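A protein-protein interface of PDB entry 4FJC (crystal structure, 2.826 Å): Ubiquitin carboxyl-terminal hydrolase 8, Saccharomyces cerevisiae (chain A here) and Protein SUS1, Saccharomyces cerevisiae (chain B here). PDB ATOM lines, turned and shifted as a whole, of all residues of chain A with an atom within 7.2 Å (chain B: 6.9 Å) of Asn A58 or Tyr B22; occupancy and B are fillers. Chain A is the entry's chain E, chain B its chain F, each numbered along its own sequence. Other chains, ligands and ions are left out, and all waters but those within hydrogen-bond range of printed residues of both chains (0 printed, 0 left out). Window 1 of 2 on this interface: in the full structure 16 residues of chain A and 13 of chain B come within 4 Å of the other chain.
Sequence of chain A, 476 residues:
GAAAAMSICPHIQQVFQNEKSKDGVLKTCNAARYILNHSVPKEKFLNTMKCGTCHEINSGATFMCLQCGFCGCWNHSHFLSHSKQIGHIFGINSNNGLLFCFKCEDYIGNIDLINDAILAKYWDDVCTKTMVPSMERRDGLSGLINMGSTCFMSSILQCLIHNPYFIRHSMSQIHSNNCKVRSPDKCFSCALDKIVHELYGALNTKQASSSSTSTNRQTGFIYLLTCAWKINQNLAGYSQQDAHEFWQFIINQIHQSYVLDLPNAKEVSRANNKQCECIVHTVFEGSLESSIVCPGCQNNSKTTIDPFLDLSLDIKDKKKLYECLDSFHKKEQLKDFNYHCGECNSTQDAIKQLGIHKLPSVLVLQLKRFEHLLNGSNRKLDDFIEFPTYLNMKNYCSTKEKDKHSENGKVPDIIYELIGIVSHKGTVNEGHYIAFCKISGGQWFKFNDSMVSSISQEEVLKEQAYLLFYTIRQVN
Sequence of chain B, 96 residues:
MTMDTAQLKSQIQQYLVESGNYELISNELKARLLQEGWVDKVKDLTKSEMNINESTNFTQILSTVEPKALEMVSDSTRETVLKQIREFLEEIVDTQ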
ATOM      1  N   PRO A  41       1.537  17.879   6.462  1.00  0.00           N
ATOM      2  CA  PRO A  41       1.766  16.522   7.004  1.00  0.00           C
ATOM      3  C   PRO A  41       0.666  15.991   7.938  1.00  0.00           C
ATOM      4  O   PRO A  41       0.138  14.905   7.701  1.00  0.00           O
ATOM      5  CB  PRO A  41       3.090  16.664   7.760  1.00  0.00           C
ATOM      6  CG  PRO A  41       3.802  17.794   7.094  1.00  0.00           C
ATOM      7  CD  PRO A  41       2.775  18.688   6.450  1.00  0.00           C
ATOM      8  N   LYS A  42       0.321  16.739   8.984  1.00  0.00           N
ATOM      9  CA  LYS A  42      -0.698  16.278   9.949  1.00  0.00           C
ATOM     10  C   LYS A  42      -2.058  16.055   9.281  1.00  0.00           C
ATOM     11  O   LYS A  42      -2.712  15.030   9.488  1.00  0.00           O
ATOM     12  CB  LYS A  42      -0.838  17.271  11.120  1.00  0.00           C
ATOM     13  CG  LYS A  42       0.136  17.027  12.274  1.00  0.00           C
ATOM     14  CD  LYS A  42       0.738  18.307  12.873  1.00  0.00           C
ATOM     15  CE  LYS A  42       1.597  18.001  14.112  1.00  0.00           C
ATOM     16  NZ  LYS A  42       2.811  18.871  14.303  1.00  0.00           N
ATOM     17  N   LYS A  44      -2.682  15.416   6.219  1.00  0.00           N
ATOM     18  CA  LYS A  44      -2.632  14.334   5.255  1.00  0.00           C
ATOM     19  C   LYS A  44      -2.773  13.014   5.962  1.00  0.00           C
ATOM     20  O   LYS A  44      -3.478  12.129   5.503  1.00  0.00           O
ATOM     21  CB  LYS A  44      -1.307  14.396   4.508  1.00  0.00           C
ATOM     22  CG  LYS A  44      -1.200  13.520   3.276  1.00  0.00           C
ATOM     23  CD  LYS A  44       0.134  13.788   2.573  1.00  0.00           C
ATOM     24  CE  LYS A  44       0.256  13.050   1.250  1.00  0.00           C
ATOM     25  NZ  LYS A  44       1.684  12.793   0.929  1.00  0.00           N
ATOM     26  N   PHE A  45      -2.108  12.883   7.099  1.00  0.00           N
ATOM     27  CA  PHE A  45      -2.174  11.637   7.847  1.00  0.00           C
ATOM     28  C   PHE A  45      -3.599  11.321   8.255  1.00  0.00           C
ATOM     29  O   PHE A  45      -4.051  10.176   8.134  1.00  0.00           O
ATOM     30  CB  PHE A  45      -1.312  11.697   9.117  1.00  0.00           C
ATOM     31  CG  PHE A  45       0.176  11.588   8.872  1.00  0.00           C
ATOM     32  CD1 PHE A  45       0.731  10.410   8.383  1.00  0.00           C
ATOM     33  CD2 PHE A  45       1.024  12.640   9.188  1.00  0.00           C
ATOM     34  CE1 PHE A  45       2.092  10.305   8.184  1.00  0.00           C
ATOM     35  CE2 PHE A  45       2.384  12.537   8.987  1.00  0.00           C
ATOM     36  CZ  PHE A  45       2.919  11.375   8.486  1.00  0.00           C
ATOM     37  N   THR A  48      -6.278  11.623   4.540  1.00  0.00           N
ATOM     38  CA  THR A  48      -6.063  10.686   3.443  1.00  0.00           C
ATOM     39  C   THR A  48      -5.512   9.333   3.880  1.00  0.00           C
ATOM     40  O   THR A  48      -5.642   8.363   3.140  1.00  0.00           O
ATOM     41  CB  THR A  48      -5.191  11.271   2.295  1.00  0.00           C
ATOM     42  OG1 THR A  48      -3.796  11.206   2.628  1.00  0.00           O
ATOM     43  CG2 THR A  48      -5.621  12.700   1.948  1.00  0.00           C
ATOM     44  N   MET A  49      -4.939   9.247   5.073  1.00  0.00           N
ATOM     45  CA  MET A  49      -4.263   8.013   5.511  1.00  0.00           C
ATOM     46  C   MET A  49      -4.855   7.452   6.799  1.00  0.00           C
ATOM     47  O   MET A  49      -4.131   6.944   7.659  1.00  0.00           O
ATOM     48  CB  MET A  49      -2.763   8.275   5.671  1.00  0.00           C
ATOM     49  CG  MET A  49      -2.068   8.530   4.349  1.00  0.00           C
ATOM     50  SD  MET A  49      -0.379   9.105   4.547  1.00  0.00           S
ATOM     51  CE  MET A  49       0.122   9.360   2.850  1.00  0.00           C
ATOM     52  N   LYS A  50      -6.184   7.558   6.899  1.00  0.00           N
ATOM     53  CA  LYS A  50      -6.981   7.064   8.038  1.00  0.00           C
ATOM     54  C   LYS A  50      -8.201   6.317   7.514  1.00  0.00           C
ATOM     55  O   LYS A  50      -9.143   6.926   6.980  1.00  0.00           O
ATOM     56  CB  LYS A  50      -7.425   8.226   8.914  1.00  0.00           C
ATOM     57  CG  LYS A  50      -8.277   7.866  10.134  1.00  0.00           C
ATOM     58  CD  LYS A  50      -8.290   9.050  11.110  1.00  0.00           C
ATOM     59  CE  LYS A  50      -9.443   9.020  12.090  1.00  0.00           C
ATOM     60  NZ  LYS A  50      -9.215  10.019  13.169  1.00  0.00           N
ATOM     61  N   CYS A  51      -8.161   4.994   7.673  1.00  0.00           N
ATOM     62  CA  CYS A  51      -9.203   4.086   7.176  1.00  0.00           C
ATOM     63  C   CYS A  51     -10.484   4.386   7.893  1.00  0.00           C
ATOM     64  O   CYS A  51     -10.481   4.550   9.100  1.00  0.00           O
ATOM     65  CB  CYS A  51      -8.800   2.644   7.449  1.00  0.00           C
ATOM     66  SG  CYS A  51      -9.910   1.362   6.862  1.00  0.00           S
ATOM     67  N   HIS A  55     -10.088   2.896  11.475  1.00  0.00           N
ATOM     68  CA  HIS A  55      -9.571   4.156  12.078  1.00  0.00           C
ATOM     69  C   HIS A  55      -8.069   4.238  12.296  1.00  0.00           C
ATOM     70  O   HIS A  55      -7.557   5.250  12.811  1.00  0.00           O
ATOM     71  CB  HIS A  55     -10.331   4.520  13.339  1.00  0.00           C
ATOM     72  CG  HIS A  55     -11.818   4.569  13.142  1.00  0.00           C
ATOM     73  ND1 HIS A  55     -12.392   5.350  12.215  1.00  0.00           N
ATOM     74  CD2 HIS A  55     -12.858   3.897  13.797  1.00  0.00           C
ATOM     75  CE1 HIS A  55     -13.736   5.187  12.262  1.00  0.00           C
ATOM     76  NE2 HIS A  55     -14.016   4.298  13.234  1.00  0.00           N
ATOM     77  N   GLU A  56      -7.342   3.208  11.864  1.00  0.00           N
ATOM     78  CA  GLU A  56      -5.884   3.207  11.986  1.00  0.00           C
ATOM     79  C   GLU A  56      -5.200   4.128  10.972  1.00  0.00           C
ATOM     80  O   GLU A  56      -5.734   4.404   9.896  1.00  0.00           O
ATOM     81  CB  GLU A  56      -5.329   1.785  11.832  1.00  0.00           C
ATOM     82  CG  GLU A  56      -5.579   0.897  13.034  1.00  0.00           C
ATOM     83  CD  GLU A  56      -5.012  -0.490  12.841  1.00  0.00           C
ATOM     84  OE1 GLU A  56      -3.877  -0.620  12.310  1.00  0.00           O
ATOM     85  OE2 GLU A  56      -5.709  -1.452  13.223  1.00  0.00           O
ATOM     86  N   ILE A  57      -4.001   4.574  11.317  1.00  0.00           N
ATOM     87  CA  ILE A  57      -3.205   5.368  10.403  1.00  0.00           C
ATOM     88  C   ILE A  57      -2.150   4.491   9.762  1.00  0.00           C
ATOM     89  O   ILE A  57      -1.481   3.733  10.426  1.00  0.00           O
ATOM     90  CB  ILE A  57      -2.521   6.558  11.102  1.00  0.00           C
ATOM     91  CG1 ILE A  57      -3.541   7.352  11.932  1.00  0.00           C
ATOM     92  CG2 ILE A  57      -1.832   7.444  10.068  1.00  0.00           C
ATOM     93  CD1 ILE A  57      -4.589   8.050  11.103  1.00  0.00           C
ATOM     94  N   ASN A  58      -2.018   4.599   8.454  1.00  0.00           N
ATOM     95  CA  ASN A  58      -1.006   3.860   7.728  1.00  0.00           C
ATOM     96  C   ASN A  58      -1.076   2.372   8.005  1.00  0.00           C
ATOM     97  O   ASN A  58      -0.047   1.701   8.102  1.00  0.00           O
ATOM     98  CB  ASN A  58       0.407   4.423   8.031  1.00  0.00           C
ATOM     99  CG  ASN A  58       0.711   5.691   7.255  1.00  0.00           C
ATOM    100  OD1 ASN A  58       1.611   6.437   7.613  1.00  0.00           O
ATOM    101  ND2 ASN A  58      -0.042   5.940   6.187  1.00  0.00           N
ATOM    102  N   SER A  59      -2.294   1.850   8.118  1.00  0.00           N
ATOM    103  CA  SER A  59      -2.504   0.408   8.105  1.00  0.00           C
ATOM    104  C   SER A  59      -2.214  -0.069   6.689  1.00  0.00           C
ATOM    105  O   SER A  59      -3.111  -0.435   5.953  1.00  0.00           O
ATOM    106  CB  SER A  59      -3.936   0.060   8.528  1.00  0.00           C
ATOM    107  OG  SER A  59      -4.260  -1.287   8.207  1.00  0.00           O
ATOM    108  N   GLY A  60      -0.937  -0.050   6.323  1.00  0.00           N
ATOM    109  CA  GLY A  60      -0.506  -0.245   4.939  1.00  0.00           C
ATOM    110  C   GLY A  60      -0.914   0.929   4.068  1.00  0.00           C
ATOM    111  O   GLY A  60      -1.196   2.016   4.579  1.00  0.00           O
ATOM    112  N   ALA A  61      -0.964   0.719   2.755  1.00  0.00           N
ATOM    113  CA  ALA A  61      -1.561   1.728   1.895  1.00  0.00           C
ATOM    114  C   ALA A  61      -2.909   2.175   2.466  1.00  0.00           C
ATOM    115  O   ALA A  61      -3.548   1.467   3.252  1.00  0.00           O
ATOM    116  CB  ALA A  61      -1.745   1.210   0.488  1.00  0.00           C
ATOM    117  N   THR A  62      -3.325   3.371   2.075  1.00  0.00           N
ATOM    118  CA  THR A  62      -4.690   3.838   2.329  1.00  0.00           C
ATOM    119  C   THR A  62      -5.250   4.475   1.043  1.00  0.00           C
ATOM    120  O   THR A  62      -4.757   5.510   0.581  1.00  0.00           O
ATOM    121  CB  THR A  62      -4.704   4.777   3.544  1.00  0.00           C
ATOM    122  OG1 THR A  62      -4.355   4.005   4.699  1.00  0.00           O
ATOM    123  CG2 THR A  62      -6.073   5.401   3.755  1.00  0.00           C
ATOM    124  N   CYS A  73      -8.118   1.034   4.222  1.00  0.00           N
ATOM    125  CA  CYS A  73      -6.791   0.419   4.420  1.00  0.00           C
ATOM    126  C   CYS A  73      -6.581  -0.867   3.608  1.00  0.00           C
ATOM    127  O   CYS A  73      -7.528  -1.536   3.216  1.00  0.00           O
ATOM    128  CB  CYS A  73      -6.478   0.188   5.900  1.00  0.00           C
ATOM    129  SG  CYS A  73      -7.312  -1.175   6.707  1.00  0.00           S
ATOM    130  N   ASN A  75      -4.089  -3.194   4.732  1.00  0.00           N
ATOM    131  CA  ASN A  75      -3.639  -4.192   5.695  1.00  0.00           C
ATOM    132  C   ASN A  75      -4.784  -5.038   6.276  1.00  0.00           C
ATOM    133  O   ASN A  75      -4.615  -6.241   6.468  1.00  0.00           O
ATOM    134  CB  ASN A  75      -2.823  -3.526   6.829  1.00  0.00           C
ATOM    135  CG  ASN A  75      -1.314  -3.438   6.544  1.00  0.00           C
ATOM    136  OD1 ASN A  75      -0.552  -3.051   7.415  1.00  0.00           O
ATOM    137  ND2 ASN A  75      -0.887  -3.802   5.348  1.00  0.00           N
ATOM    138  N   SER A  94      -2.772   6.963  -1.348  1.00  0.00           N
ATOM    139  CA  SER A  94      -2.403   8.324  -0.901  1.00  0.00           C
ATOM    140  C   SER A  94      -0.905   8.588  -0.746  1.00  0.00           C
ATOM    141  O   SER A  94      -0.554   9.722  -0.453  1.00  0.00           O
ATOM    142  CB  SER A  94      -3.115   8.714   0.424  1.00  0.00           C
ATOM    143  OG  SER A  94      -3.228   7.634   1.338  1.00  0.00           O
ATOM    144  N   ASN A  95      -0.030   7.583  -0.895  1.00  0.00           N
ATOM    145  CA  ASN A  95       1.424   7.834  -0.770  1.00  0.00           C
ATOM    146  C   ASN A  95       1.919   8.398  -2.089  1.00  0.00           C
ATOM    147  O   ASN A  95       2.259   9.553  -2.186  1.00  0.00           O
ATOM    148  CB  ASN A  95       2.227   6.575  -0.368  1.00  0.00           C
ATOM    149  CG  ASN A  95       1.974   6.121   1.076  1.00  0.00           C
ATOM    150  OD1 ASN A  95       2.117   6.890   2.026  1.00  0.00           O
ATOM    151  ND2 ASN A  95       1.610   4.838   1.236  1.00  0.00           N
ATOM    152  N   GLN B  13      -2.632   6.604  18.036  1.00  0.00           N
ATOM    153  CA  GLN B  13      -2.138   7.091  16.757  1.00  0.00           C
ATOM    154  C   GLN B  13      -2.588   8.518  16.492  1.00  0.00           C
ATOM    155  O   GLN B  13      -1.756   9.392  16.262  1.00  0.00           O
ATOM    156  CB  GLN B  13      -2.603   6.172  15.636  1.00  0.00           C
ATOM    157  CG  GLN B  13      -2.079   4.756  15.794  1.00  0.00           C
ATOM    158  CD  GLN B  13      -2.148   3.959  14.513  1.00  0.00           C
ATOM    159  OE1 GLN B  13      -3.233   3.621  14.046  1.00  0.00           O
ATOM    160  NE2 GLN B  13      -0.981   3.649  13.935  1.00  0.00           N
ATOM    161  N   TYR B  15      -3.383  10.749  18.456  1.00  0.00           N
ATOM    162  CA  TYR B  15      -2.704  11.655  19.407  1.00  0.00           C
ATOM    163  C   TYR B  15      -1.177  11.786  19.197  1.00  0.00           C
ATOM    164  O   TYR B  15      -0.523  12.585  19.875  1.00  0.00           O
ATOM    165  CB  TYR B  15      -3.015  11.221  20.849  1.00  0.00           C
ATOM    166  CG  TYR B  15      -4.468  11.464  21.280  1.00  0.00           C
ATOM    167  CD1 TYR B  15      -5.518  11.439  20.356  1.00  0.00           C
ATOM    168  CD2 TYR B  15      -4.786  11.737  22.608  1.00  0.00           C
ATOM    169  CE1 TYR B  15      -6.824  11.660  20.743  1.00  0.00           C
ATOM    170  CE2 TYR B  15      -6.094  11.957  23.000  1.00  0.00           C
ATOM    171  CZ  TYR B  15      -7.107  11.916  22.059  1.00  0.00           C
ATOM    172  OH  TYR B  15      -8.417  12.136  22.425  1.00  0.00           O
ATOM    173  N   LEU B  16      -0.626  10.993  18.271  1.00  0.00           N
ATOM    174  CA  LEU B  16       0.777  11.103  17.845  1.00  0.00           C
ATOM    175  C   LEU B  16       0.893  12.033  16.657  1.00  0.00           C
ATOM    176  O   LEU B  16       1.788  12.865  16.603  1.00  0.00           O
ATOM    177  CB  LEU B  16       1.327   9.747  17.409  1.00  0.00           C
ATOM    178  CG  LEU B  16       1.815   8.795  18.480  1.00  0.00           C
ATOM    179  CD1 LEU B  16       2.073   7.440  17.836  1.00  0.00           C
ATOM    180  CD2 LEU B  16       3.055   9.372  19.151  1.00  0.00           C
ATOM    181  N   VAL B  17       0.011  11.852  15.677  1.00  0.00           N
ATOM    182  CA  VAL B  17      -0.046  12.763  14.549  1.00  0.00           C
ATOM    183  C   VAL B  17      -0.210  14.166  15.095  1.00  0.00           C
ATOM    184  O   VAL B  17       0.566  15.046  14.743  1.00  0.00           O
ATOM    185  CB  VAL B  17      -1.213  12.453  13.601  1.00  0.00           C
ATOM    186  CG1 VAL B  17      -1.343  13.540  12.539  1.00  0.00           C
ATOM    187  CG2 VAL B  17      -1.015  11.086  12.973  1.00  0.00           C
ATOM    188  N   GLU B  18      -1.188  14.346  15.988  1.00  0.00           N
ATOM    189  CA  GLU B  18      -1.460  15.645  16.615  1.00  0.00           C
ATOM    190  C   GLU B  18      -0.277  16.240  17.379  1.00  0.00           C
ATOM    191  O   GLU B  18       0.001  17.431  17.265  1.00  0.00           O
ATOM    192  CB  GLU B  18      -2.658  15.536  17.557  1.00  0.00           C
ATOM    193  CG  GLU B  18      -3.994  15.312  16.854  1.00  0.00           C
ATOM    194  CD  GLU B  18      -4.458  16.498  16.008  1.00  0.00           C
ATOM    195  OE1 GLU B  18      -3.681  17.478  15.851  1.00  0.00           O
ATOM    196  OE2 GLU B  18      -5.613  16.441  15.500  1.00  0.00           O
ATOM    197  N   SER B  19       0.422  15.410  18.143  1.00  0.00           N
ATOM    198  CA  SER B  19       1.604  15.856  18.872  1.00  0.00           C
ATOM    199  C   SER B  19       2.792  16.124  17.962  1.00  0.00           C
ATOM    200  O   SER B  19       3.827  16.589  18.410  1.00  0.00           O
ATOM    201  CB  SER B  19       2.004  14.801  19.892  1.00  0.00           C
ATOM    202  OG  SER B  19       2.392  13.601  19.246  1.00  0.00           O
ATOM    203  N   GLY B  20       2.657  15.790  16.683  1.00  0.00           N
ATOM    204  CA  GLY B  20       3.725  15.979  15.713  1.00  0.00           C
ATOM    205  C   GLY B  20       4.845  14.981  15.837  1.00  0.00           C
ATOM    206  O   GLY B  20       5.855  15.102  15.143  1.00  0.00           O
ATOM    207  N   ASN B  21       4.663  13.985  16.696  1.00  0.00           N
ATOM    208  CA  ASN B  21       5.644  12.916  16.850  1.00  0.00           C
ATOM    209  C   ASN B  21       5.496  11.778  15.846  1.00  0.00           C
ATOM    210  O   ASN B  21       6.399  10.949  15.717  1.00  0.00           O
ATOM    211  CB  ASN B  21       5.590  12.339  18.259  1.00  0.00           C
ATOM    212  CG  ASN B  21       6.037  13.328  19.298  1.00  0.00           C
ATOM    213  OD1 ASN B  21       5.318  14.263  19.623  1.00  0.00           O
ATOM    214  ND2 ASN B  21       7.226  13.125  19.821  1.00  0.00           N
ATOM    215  N   TYR B  22       4.372  11.722  15.142  1.00  0.00           N
ATOM    216  CA  TYR B  22       4.215  10.731  14.079  1.00  0.00           C
ATOM    217  C   TYR B  22       5.184  11.054  12.936  1.00  0.00           C
ATOM    218  O   TYR B  22       5.944  10.165  12.496  1.00  0.00           O
ATOM    219  CB  TYR B  22       2.767  10.667  13.578  1.00  0.00           C
ATOM    220  CG  TYR B  22       2.469   9.393  12.847  1.00  0.00           C
ATOM    221  CD1 TYR B  22       2.320   8.193  13.531  1.00  0.00           C
ATOM    222  CD2 TYR B  22       2.355   9.379  11.471  1.00  0.00           C
ATOM    223  CE1 TYR B  22       2.056   7.010  12.859  1.00  0.00           C
ATOM    224  CE2 TYR B  22       2.096   8.208  10.787  1.00  0.00           C
ATOM    225  CZ  TYR B  22       1.945   7.030  11.485  1.00  0.00           C
ATOM    226  OH  TYR B  22       1.684   5.877  10.782  1.00  0.00           O
ATOM    227  N   GLU B  23       5.168  12.319  12.493  1.00  0.00           N
ATOM    228  CA  GLU B  23       6.144  12.835  11.519  1.00  0.00           C
ATOM    229  C   GLU B  23       7.617  12.577  11.922  1.00  0.00           C
ATOM    230  O   GLU B  23       8.359  11.948  11.170  1.00  0.00           O
ATOM    231  CB  GLU B  23       5.993  14.333  11.330  1.00  0.00           C
ATOM    232  CG  GLU B  23       4.650  14.818  10.854  1.00  0.00           C
ATOM    233  CD  GLU B  23       4.447  16.293  11.140  1.00  0.00           C
ATOM    234  OE1 GLU B  23       5.187  17.104  10.532  1.00  0.00           O
ATOM    235  OE2 GLU B  23       3.549  16.625  11.959  1.00  0.00           O
ATOM    236  N   LEU B  24       8.052  13.068  13.084  1.00  0.00           N
ATOM    237  CA  LEU B  24       9.405  12.738  13.576  1.00  0.00           C
ATOM    238  C   LEU B  24       9.726  11.246  13.359  1.00  0.00           C
ATOM    239  O   LEU B  24      10.759  10.911  12.777  1.00  0.00           O
ATOM    240  CB  LEU B  24       9.588  13.098  15.061  1.00  0.00           C
ATOM    241  CG  LEU B  24       9.940  14.536  15.478  1.00  0.00           C
ATOM    242  CD1 LEU B  24       8.812  15.537  15.226  1.00  0.00           C
ATOM    243  CD2 LEU B  24      10.321  14.556  16.953  1.00  0.00           C
ATOM    244  N   ILE B  25       8.838  10.359  13.804  1.00  0.00           N
ATOM    245  CA  ILE B  25       9.107   8.928  13.697  1.00  0.00           C
ATOM    246  C   ILE B  25       9.162   8.536  12.238  1.00  0.00           C
ATOM    247  O   ILE B  25      10.089   7.860  11.816  1.00  0.00           O
ATOM    248  CB  ILE B  25       8.025   8.053  14.365  1.00  0.00           C
ATOM    249  CG1 ILE B  25       8.090   8.149  15.878  1.00  0.00           C
ATOM    250  CG2 ILE B  25       8.170   6.577  13.979  1.00  0.00           C
ATOM    251  CD1 ILE B  25       6.908   7.460  16.520  1.00  0.00           C
ATOM    252  N   SER B  26       8.148   8.943  11.479  1.00  0.00           N
ATOM    253  CA  SER B  26       8.001   8.497  10.087  1.00  0.00           C
ATOM    254  C   SER B  26       9.211   8.889   9.235  1.00  0.00           C
ATOM    255  O   SER B  26       9.668   8.124   8.393  1.00  0.00           O
ATOM    256  CB  SER B  26       6.721   9.067   9.481  1.00  0.00           C
ATOM    257  OG  SER B  26       6.619   8.719   8.119  1.00  0.00           O
ATOM    258  N   ASN B  27       9.737  10.076   9.483  1.00  0.00           N
ATOM    259  CA  ASN B  27      10.876  10.565   8.743  1.00  0.00           C
ATOM    260  C   ASN B  27      12.184   9.982   9.259  1.00  0.00           C
ATOM    261  O   ASN B  27      13.098   9.687   8.476  1.00  0.00           O
ATOM    262  CB  ASN B  27      10.910  12.088   8.814  1.00  0.00           C
ATOM    263  CG  ASN B  27       9.761  12.722   8.066  1.00  0.00           C
ATOM    264  OD1 ASN B  27       9.291  13.791   8.441  1.00  0.00           O
ATOM    265  ND2 ASN B  27       9.299  12.063   7.002  1.00  0.00           N
ATOM    266  N   GLU B  28      12.286   9.813  10.570  1.00  0.00           N
ATOM    267  CA  GLU B  28      13.476   9.199  11.116  1.00  0.00           C
ATOM    268  C   GLU B  28      13.600   7.800  10.553  1.00  0.00           C
ATOM    269  O   GLU B  28      14.687   7.346  10.248  1.00  0.00           O
ATOM    270  CB  GLU B  28      13.422   9.113  12.628  1.00  0.00           C
ATOM    271  CG  GLU B  28      14.793   8.908  13.262  1.00  0.00           C
ATOM    272  CD  GLU B  28      15.314  10.143  13.977  1.00  0.00           C
ATOM    273  OE1 GLU B  28      16.269   9.967  14.766  1.00  0.00           O
ATOM    274  OE2 GLU B  28      14.764  11.267  13.773  1.00  0.00           O
ATOM    275  N   PHE B  88       7.887   7.882  23.290  1.00  0.00           N
ATOM    276  CA  PHE B  88       6.735   8.726  22.972  1.00  0.00           C
ATOM    277  C   PHE B  88       5.419   8.175  23.525  1.00  0.00           C
ATOM    278  O   PHE B  88       4.480   8.941  23.755  1.00  0.00           O
ATOM    279  CB  PHE B  88       6.599   8.945  21.456  1.00  0.00           C
ATOM    280  CG  PHE B  88       7.712   9.750  20.839  1.00  0.00           C
ATOM    281  CD1 PHE B  88       8.310  10.802  21.522  1.00  0.00           C
ATOM    282  CD2 PHE B  88       8.157   9.450  19.559  1.00  0.00           C
ATOM    283  CE1 PHE B  88       9.336  11.532  20.943  1.00  0.00           C
ATOM    284  CE2 PHE B  88       9.174  10.183  18.969  1.00  0.00           C
ATOM    285  CZ  PHE B  88       9.768  11.225  19.663  1.00  0.00           C
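O of Met A49 is in hydrogen-bond range of N of Asn A58, 3.3 Å away. O of Glu A56 is in hydrogen-bond range of N of Cys A51. N of Tyr B22 lies within hydrogen-bond range of O of Leu B16 (3.2 Å). The backbone carbonyl oxygen (O) of Glu B23 lies close to the side-chain amide oxygen (OD1) of Asn B27.
Among the printed residues, merely in contact across the chains: Pro A41 with Glu B23 (3.5 Å), Lys A42 with Val B17 (3.2 Å), Lys A42 with Glu B18 (3.6 Å), Lys A42 with Gly B20 (3.3 Å), Phe A45 with Val B17 (3.9 Å), Phe A45 with Tyr B22 (3.3 Å), Phe A45 with Glu B23 (3.7 Å), Glu A56 with Gln B13 (3.4 Å) and Ile A57 with Tyr B22 (3.8 Å).
The side-chain carboxylate (OE2) of Glu B23 is in salt-bridge range of the side-chain amino group (NZ) of Lys A42 (3.3 Å). The backbone NH (N) of Ile A57 sits at hydrogen-bond distance from the side-chain amide oxygen (OE1) of Gln B13, 3.0 Å away. OD1 of Asn A58 lies within hydrogen-bond range of OH of Tyr B22.
Hydrophobic or aromatic side chains of chain B that line the printed part of chain A: Val B17 and Tyr B22. Of the 20 printed residues of chain A, 6 touch a printed residue of chain B. Hydrophobic or aromatic side chains of chain A that line the printed part of chain B: Pro A41, Phe A45 and Ile A57. Among the printed residues, 12 pairs touch across the chains. Among the printed residues, Asp or Glu carboxylates within 4 Å of a Lys or Arg side-chain nitrogen of the other chain: Lys A42 with Glu B23 (3.3 Å).
Printed residues of chain B within 4 Å of Ile A57: Gln B13 (3.0 Å) and Tyr B22 (3.8 Å). Of chain B, only Tyr B22 (3.2 Å) comes within 4 Å of Asn A58. Ala A61 touches none of the printed residues of chain B. Of the printed residues of chain A, Glu B18 touches Lys A42 (3.6 Å). Printed residues of chain A within 4 Å of Gly B20: Lys A42. Phe B88 touches none of the printed residues of chain A. The nearest residue of chain B that does not touch Asn A58 is Ser B26 (5.5 Å). The nearest printed residue of chain A that does not touch Glu B23 is Asn A58 (8.4 Å).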
